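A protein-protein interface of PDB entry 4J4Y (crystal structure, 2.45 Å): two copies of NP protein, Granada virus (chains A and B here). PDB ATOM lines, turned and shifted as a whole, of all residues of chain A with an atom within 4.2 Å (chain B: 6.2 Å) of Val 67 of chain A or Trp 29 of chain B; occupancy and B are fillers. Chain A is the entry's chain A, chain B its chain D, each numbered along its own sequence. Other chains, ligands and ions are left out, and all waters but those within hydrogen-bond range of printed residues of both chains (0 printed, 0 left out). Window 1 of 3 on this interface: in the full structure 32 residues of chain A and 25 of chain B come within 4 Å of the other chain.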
ATOM      1  N   LYS A  63     -18.667  20.134 -14.511  1.00  0.00           N
ATOM      2  CA  LYS A  63     -19.111  21.360 -13.922  1.00  0.00           C
ATOM      3  C   LYS A  63     -19.181  22.488 -14.931  1.00  0.00           C
ATOM      4  O   LYS A  63     -20.115  23.242 -14.956  1.00  0.00           O
ATOM      5  CB  LYS A  63     -18.174  21.746 -12.812  1.00  0.00           C
ATOM      6  CG  LYS A  63     -18.410  21.046 -11.514  1.00  0.00           C
ATOM      7  CD  LYS A  63     -17.301  21.301 -10.538  1.00  0.00           C
ATOM      8  CE  LYS A  63     -17.471  20.414  -9.347  1.00  0.00           C
ATOM      9  NZ  LYS A  63     -16.507  20.684  -8.266  1.00  0.00           N
ATOM     10  N   MET A  64     -18.175  22.587 -15.762  1.00  0.00           N
ATOM     11  CA  MET A  64     -18.203  23.518 -16.832  1.00  0.00           C
ATOM     12  C   MET A  64     -19.276  23.275 -17.848  1.00  0.00           C
ATOM     13  O   MET A  64     -19.908  24.196 -18.276  1.00  0.00           O
ATOM     14  CB  MET A  64     -16.857  23.561 -17.483  1.00  0.00           C
ATOM     15  CG  MET A  64     -15.878  24.231 -16.587  1.00  0.00           C
ATOM     16  SD  MET A  64     -14.270  24.294 -17.289  1.00  0.00           S
ATOM     17  CE  MET A  64     -13.820  25.938 -16.893  1.00  0.00           C
ATOM     18  N   MET A  65     -19.483  22.039 -18.220  1.00  0.00           N
ATOM     19  CA  MET A  65     -20.473  21.735 -19.190  1.00  0.00           C
ATOM     20  C   MET A  65     -21.843  22.116 -18.674  1.00  0.00           C
ATOM     21  O   MET A  65     -22.678  22.530 -19.423  1.00  0.00           O
ATOM     22  CB  MET A  65     -20.403  20.278 -19.577  1.00  0.00           C
ATOM     23  CG  MET A  65     -19.231  19.931 -20.463  1.00  0.00           C
ATOM     24  SD  MET A  65     -19.330  18.358 -21.274  1.00  0.00           S
ATOM     25  CE  MET A  65     -18.830  17.297 -19.969  1.00  0.00           C
ATOM     26  N   ILE A  66     -22.080  21.923 -17.391  1.00  0.00           N
ATOM     27  CA  ILE A  66     -23.314  22.313 -16.781  1.00  0.00           C
ATOM     28  C   ILE A  66     -23.525  23.804 -16.742  1.00  0.00           C
ATOM     29  O   ILE A  66     -24.590  24.279 -17.017  1.00  0.00           O
ATOM     30  CB  ILE A  66     -23.449  21.698 -15.395  1.00  0.00           C
ATOM     31  CG1 ILE A  66     -23.546  20.198 -15.524  1.00  0.00           C
ATOM     32  CG2 ILE A  66     -24.691  22.201 -14.690  1.00  0.00           C
ATOM     33  CD1 ILE A  66     -23.547  19.480 -14.219  1.00  0.00           C
ATOM     34  N   VAL A  67     -22.495  24.534 -16.387  1.00  0.00           N
ATOM     35  CA  VAL A  67     -22.621  25.956 -16.296  1.00  0.00           C
ATOM     36  C   VAL A  67     -22.933  26.491 -17.666  1.00  0.00           C
ATOM     37  O   VAL A  67     -23.809  27.281 -17.841  1.00  0.00           O
ATOM     38  CB  VAL A  67     -21.385  26.600 -15.666  1.00  0.00           C
ATOM     39  CG1 VAL A  67     -21.347  28.088 -15.916  1.00  0.00           C
ATOM     40  CG2 VAL A  67     -21.384  26.347 -14.189  1.00  0.00           C
ATOM     41  N   LEU A  68     -22.256  25.953 -18.641  1.00  0.00           N
ATOM     42  CA  LEU A  68     -22.448  26.331 -20.003  1.00  0.00           C
ATOM     43  C   LEU A  68     -23.847  26.084 -20.459  1.00  0.00           C
ATOM     44  O   LEU A  68     -24.424  26.895 -21.100  1.00  0.00           O
ATOM     45  CB  LEU A  68     -21.588  25.419 -20.825  1.00  0.00           C
ATOM     46  CG  LEU A  68     -20.772  25.893 -21.993  1.00  0.00           C
ATOM     47  CD1 LEU A  68     -20.303  24.638 -22.658  1.00  0.00           C
ATOM     48  CD2 LEU A  68     -21.525  26.740 -22.984  1.00  0.00           C
ATOM     49  N   ASN A  69     -24.368  24.932 -20.139  1.00  0.00           N
ATOM     50  CA  ASN A  69     -25.718  24.589 -20.483  1.00  0.00           C
ATOM     51  C   ASN A  69     -26.775  25.479 -19.836  1.00  0.00           C
ATOM     52  O   ASN A  69     -27.715  25.856 -20.468  1.00  0.00           O
ATOM     53  CB  ASN A  69     -25.947  23.132 -20.154  1.00  0.00           C
ATOM     54  CG  ASN A  69     -27.355  22.688 -20.370  1.00  0.00           C
ATOM     55  OD1 ASN A  69     -27.976  22.219 -19.476  1.00  0.00           O
ATOM     56  ND2 ASN A  69     -27.836  22.781 -21.556  1.00  0.00           N
ATOM     57  N   LEU A  70     -26.622  25.782 -18.574  1.00  0.00           N
ATOM     58  CA  LEU A  70     -27.571  26.619 -17.928  1.00  0.00           C
ATOM     59  C   LEU A  70     -27.587  27.992 -18.518  1.00  0.00           C
ATOM     60  O   LEU A  70     -28.628  28.540 -18.762  1.00  0.00           O
ATOM     61  CB  LEU A  70     -27.209  26.757 -16.479  1.00  0.00           C
ATOM     62  CG  LEU A  70     -27.080  25.484 -15.697  1.00  0.00           C
ATOM     63  CD1 LEU A  70     -26.969  25.689 -14.215  1.00  0.00           C
ATOM     64  CD2 LEU A  70     -28.162  24.522 -16.026  1.00  0.00           C
ATOM     65  N   VAL A  71     -26.416  28.575 -18.654  1.00  0.00           N
ATOM     66  CA  VAL A  71     -26.238  29.856 -19.287  1.00  0.00           C
ATOM     67  C   VAL A  71     -26.479  29.937 -20.783  1.00  0.00           C
ATOM     68  O   VAL A  71     -27.094  30.857 -21.226  1.00  0.00           O
ATOM     69  CB  VAL A  71     -24.869  30.426 -18.902  1.00  0.00           C
ATOM     70  CG1 VAL A  71     -24.575  31.708 -19.617  1.00  0.00           C
ATOM     71  CG2 VAL A  71     -24.836  30.687 -17.420  1.00  0.00           C
ATOM     72  N   TRP A 122     -25.155  18.125  -8.856  1.00  0.00           N
ATOM     73  CA  TRP A 122     -24.443  19.373  -9.000  1.00  0.00           C
ATOM     74  C   TRP A 122     -25.279  20.552  -9.490  1.00  0.00           C
ATOM     75  O   TRP A 122     -25.145  21.643  -9.020  1.00  0.00           O
ATOM     76  CB  TRP A 122     -23.198  19.227  -9.860  1.00  0.00           C
ATOM     77  CG  TRP A 122     -22.253  20.248  -9.549  1.00  0.00           C
ATOM     78  CD1 TRP A 122     -21.485  20.305  -8.478  1.00  0.00           C
ATOM     79  CD2 TRP A 122     -21.980  21.415 -10.296  1.00  0.00           C
ATOM     80  NE1 TRP A 122     -20.736  21.414  -8.490  1.00  0.00           N
ATOM     81  CE2 TRP A 122     -21.034  22.129  -9.604  1.00  0.00           C
ATOM     82  CE3 TRP A 122     -22.465  21.934 -11.472  1.00  0.00           C
ATOM     83  CZ2 TRP A 122     -20.531  23.312 -10.054  1.00  0.00           C
ATOM     84  CZ3 TRP A 122     -21.978  23.103 -11.905  1.00  0.00           C
ATOM     85  CH2 TRP A 122     -21.015  23.782 -11.210  1.00  0.00           C
ATOM     86  N   THR B  24     -17.466  32.152  -7.051  1.00  0.00           N
ATOM     87  CA  THR B  24     -16.504  32.972  -7.727  1.00  0.00           C
ATOM     88  C   THR B  24     -15.942  32.292  -8.938  1.00  0.00           C
ATOM     89  O   THR B  24     -15.847  32.899  -9.988  1.00  0.00           O
ATOM     90  CB  THR B  24     -15.384  33.413  -6.799  1.00  0.00           C
ATOM     91  OG1 THR B  24     -14.541  32.303  -6.534  1.00  0.00           O
ATOM     92  CG2 THR B  24     -15.954  33.884  -5.518  1.00  0.00           C
ATOM     93  N   THR B  25     -15.547  31.049  -8.799  1.00  0.00           N
ATOM     94  CA  THR B  25     -15.068  30.341  -9.956  1.00  0.00           C
ATOM     95  C   THR B  25     -16.168  30.141 -10.985  1.00  0.00           C
ATOM     96  O   THR B  25     -15.937  30.293 -12.153  1.00  0.00           O
ATOM     97  CB  THR B  25     -14.220  29.082  -9.633  1.00  0.00           C
ATOM     98  OG1 THR B  25     -14.690  27.968 -10.367  1.00  0.00           O
ATOM     99  CG2 THR B  25     -14.240  28.735  -8.189  1.00  0.00           C
ATOM    100  N   ILE B  26     -17.369  29.841 -10.545  1.00  0.00           N
ATOM    101  CA  ILE B  26     -18.463  29.633 -11.468  1.00  0.00           C
ATOM    102  C   ILE B  26     -18.775  30.864 -12.274  1.00  0.00           C
ATOM    103  O   ILE B  26     -18.998  30.790 -13.454  1.00  0.00           O
ATOM    104  CB  ILE B  26     -19.735  29.197 -10.708  1.00  0.00           C
ATOM    105  CG1 ILE B  26     -19.528  27.816 -10.119  1.00  0.00           C
ATOM    106  CG2 ILE B  26     -20.964  29.175 -11.590  1.00  0.00           C
ATOM    107  CD1 ILE B  26     -20.753  27.183  -9.559  1.00  0.00           C
ATOM    108  N   ASN B  27     -18.858  31.985 -11.618  1.00  0.00           N
ATOM    109  CA  ASN B  27     -19.181  33.192 -12.303  1.00  0.00           C
ATOM    110  C   ASN B  27     -18.116  33.536 -13.286  1.00  0.00           C
ATOM    111  O   ASN B  27     -18.393  34.052 -14.341  1.00  0.00           O
ATOM    112  CB  ASN B  27     -19.450  34.290 -11.314  1.00  0.00           C
ATOM    113  CG  ASN B  27     -20.817  34.172 -10.715  1.00  0.00           C
ATOM    114  OD1 ASN B  27     -21.816  34.116 -11.420  1.00  0.00           O
ATOM    115  ND2 ASN B  27     -20.869  34.100  -9.413  1.00  0.00           N
ATOM    116  N   ALA B  28     -16.894  33.188 -12.930  1.00  0.00           N
ATOM    117  CA  ALA B  28     -15.729  33.381 -13.768  1.00  0.00           C
ATOM    118  C   ALA B  28     -15.813  32.608 -15.044  1.00  0.00           C
ATOM    119  O   ALA B  28     -15.298  33.040 -16.044  1.00  0.00           O
ATOM    120  CB  ALA B  28     -14.470  33.018 -13.028  1.00  0.00           C
ATOM    121  N   TRP B  29     -16.398  31.421 -14.982  1.00  0.00           N
ATOM    122  CA  TRP B  29     -16.730  30.654 -16.161  1.00  0.00           C
ATOM    123  C   TRP B  29     -17.814  31.321 -16.972  1.00  0.00           C
ATOM    124  O   TRP B  29     -17.739  31.427 -18.163  1.00  0.00           O
ATOM    125  CB  TRP B  29     -17.196  29.263 -15.768  1.00  0.00           C
ATOM    126  CG  TRP B  29     -16.175  28.377 -15.168  1.00  0.00           C
ATOM    127  CD1 TRP B  29     -14.845  28.469 -15.298  1.00  0.00           C
ATOM    128  CD2 TRP B  29     -16.416  27.232 -14.350  1.00  0.00           C
ATOM    129  NE1 TRP B  29     -14.237  27.481 -14.608  1.00  0.00           N
ATOM    130  CE2 TRP B  29     -15.185  26.706 -14.012  1.00  0.00           C
ATOM    131  CE3 TRP B  29     -17.557  26.611 -13.874  1.00  0.00           C
ATOM    132  CZ2 TRP B  29     -15.058  25.589 -13.235  1.00  0.00           C
ATOM    133  CZ3 TRP B  29     -17.427  25.519 -13.097  1.00  0.00           C
ATOM    134  CH2 TRP B  29     -16.196  25.009 -12.786  1.00  0.00           C
ATOM    135  N   VAL B  30     -18.847  31.769 -16.298  1.00  0.00           N
ATOM    136  CA  VAL B  30     -19.941  32.446 -16.962  1.00  0.00           C
ATOM    137  C   VAL B  30     -19.452  33.717 -17.605  1.00  0.00           C
ATOM    138  O   VAL B  30     -19.930  34.100 -18.649  1.00  0.00           O
ATOM    139  CB  VAL B  30     -21.184  32.635 -16.076  1.00  0.00           C
ATOM    140  CG1 VAL B  30     -21.269  31.528 -15.068  1.00  0.00           C
ATOM    141  CG2 VAL B  30     -21.217  33.970 -15.382  1.00  0.00           C
ATOM    142  N   ASN B  31     -18.488  34.364 -16.977  1.00  0.00           N
ATOM    143  CA  ASN B  31     -17.947  35.558 -17.559  1.00  0.00           C
ATOM    144  C   ASN B  31     -17.289  35.262 -18.885  1.00  0.00           C
ATOM    145  O   ASN B  31     -17.523  35.943 -19.843  1.00  0.00           O
ATOM    146  CB  ASN B  31     -16.993  36.226 -16.585  1.00  0.00           C
ATOM    147  CG  ASN B  31     -17.721  36.958 -15.481  1.00  0.00           C
ATOM    148  OD1 ASN B  31     -18.882  37.310 -15.626  1.00  0.00           O
ATOM    149  ND2 ASN B  31     -17.045  37.188 -14.376  1.00  0.00           N
ATOM    150  N   GLU B  32     -16.485  34.216 -18.905  1.00  0.00           N
ATOM    151  CA  GLU B  32     -15.871  33.628 -20.094  1.00  0.00           C
ATOM    152  C   GLU B  32     -16.810  32.984 -21.143  1.00  0.00           C
ATOM    153  O   GLU B  32     -16.477  32.919 -22.291  1.00  0.00           O
ATOM    154  CB  GLU B  32     -14.739  32.682 -19.692  1.00  0.00           C
ATOM    155  CG  GLU B  32     -13.372  33.331 -19.558  1.00  0.00           C
ATOM    156  CD  GLU B  32     -12.627  32.964 -18.275  1.00  0.00           C
ATOM    157  OE1 GLU B  32     -12.353  31.774 -18.032  1.00  0.00           O
ATOM    158  OE2 GLU B  32     -12.284  33.869 -17.490  1.00  0.00           O
ATOM    159  N   PHE B  33     -17.948  32.452 -20.727  1.00  0.00           N
ATOM    160  CA  PHE B  33     -18.877  31.812 -21.647  1.00  0.00           C
ATOM    161  C   PHE B  33     -19.968  32.727 -22.117  1.00  0.00           C
ATOM    162  O   PHE B  33     -20.656  32.447 -23.068  1.00  0.00           O
ATOM    163  CB  PHE B  33     -19.607  30.662 -20.969  1.00  0.00           C
ATOM    164  CG  PHE B  33     -18.768  29.470 -20.684  1.00  0.00           C
ATOM    165  CD1 PHE B  33     -17.575  29.274 -21.320  1.00  0.00           C
ATOM    166  CD2 PHE B  33     -19.194  28.539 -19.777  1.00  0.00           C
ATOM    167  CE1 PHE B  33     -16.811  28.185 -21.040  1.00  0.00           C
ATOM    168  CE2 PHE B  33     -18.438  27.442 -19.491  1.00  0.00           C
ATOM    169  CZ  PHE B  33     -17.245  27.260 -20.123  1.00  0.00           C
ATOM    170  N   ALA B  34     -20.187  33.785 -21.376  1.00  0.00           N
ATOM    171  CA  ALA B  34     -21.237  34.727 -21.669  1.00  0.00           C
ATOM    172  C   ALA B  34     -20.936  35.569 -22.872  1.00  0.00           C
ATOM    173  O   ALA B  34     -19.804  35.946 -23.086  1.00  0.00           O
ATOM    174  CB  ALA B  34     -21.434  35.625 -20.475  1.00  0.00           C
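No position is printed for both chains.
Val 67 of chain A touches three residues of chain B. Printed residues of chain A within 4 Å of Ile 26 of chain B: Val 67 (3.9 Å) and Trp 122 (3.8 Å). Of the printed residues of chain B, Leu 68 of chain A touches Phe 33. Of the printed residues of chain B, Trp 122 of chain A touches Ile 26. The nearest printed residue of chain B that does not touch Trp 122 of chain A is Trp 29 of chain B (4.4 Å).
Hydrophobic or aromatic side chains of chain B within 4 Å of the printed part of chain A: Ile 26, Trp 29, Val 30 and Phe 33. Of the 10 printed residues of chain A, 5 touch a printed residue of chain B. Printed residues of chain A that touch a printed residue of chain B: Lys 63, Met 64, Val 67, Leu 68 and Trp 122. Hydrophobic or aromatic side chains of chain A that line the printed part of chain B: Met 64, Val 67, Leu 68 and Trp 122. Among the printed residues, 8 pairs touch across the chains. Among the printed residues, no Asp or Glu carboxylate lies within 4 Å of a Lys or Arg side-chain nitrogen of the other chain.
Among the printed residues, pairs that only touch across the chains: Lys 63 of chain A with Trp 29 of chain B (3.8 Å), Met 64 of chain A with Trp 29 of chain B (2.8 Å), Met 64 of chain A with Phe 33 of chain B (3.8 Å), Val 67 of chain A with Ile 26 of chain B (3.9 Å), Val 67 of chain A with Trp 29 of chain B (3.8 Å), Val 67 of chain A with Val 30 of chain B (3.5 Å), Leu 68 of chain A with Phe 33 of chain B (3.8 Å) and Trp 122 of chain A with Ile 26 of chain B (3.8 Å).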
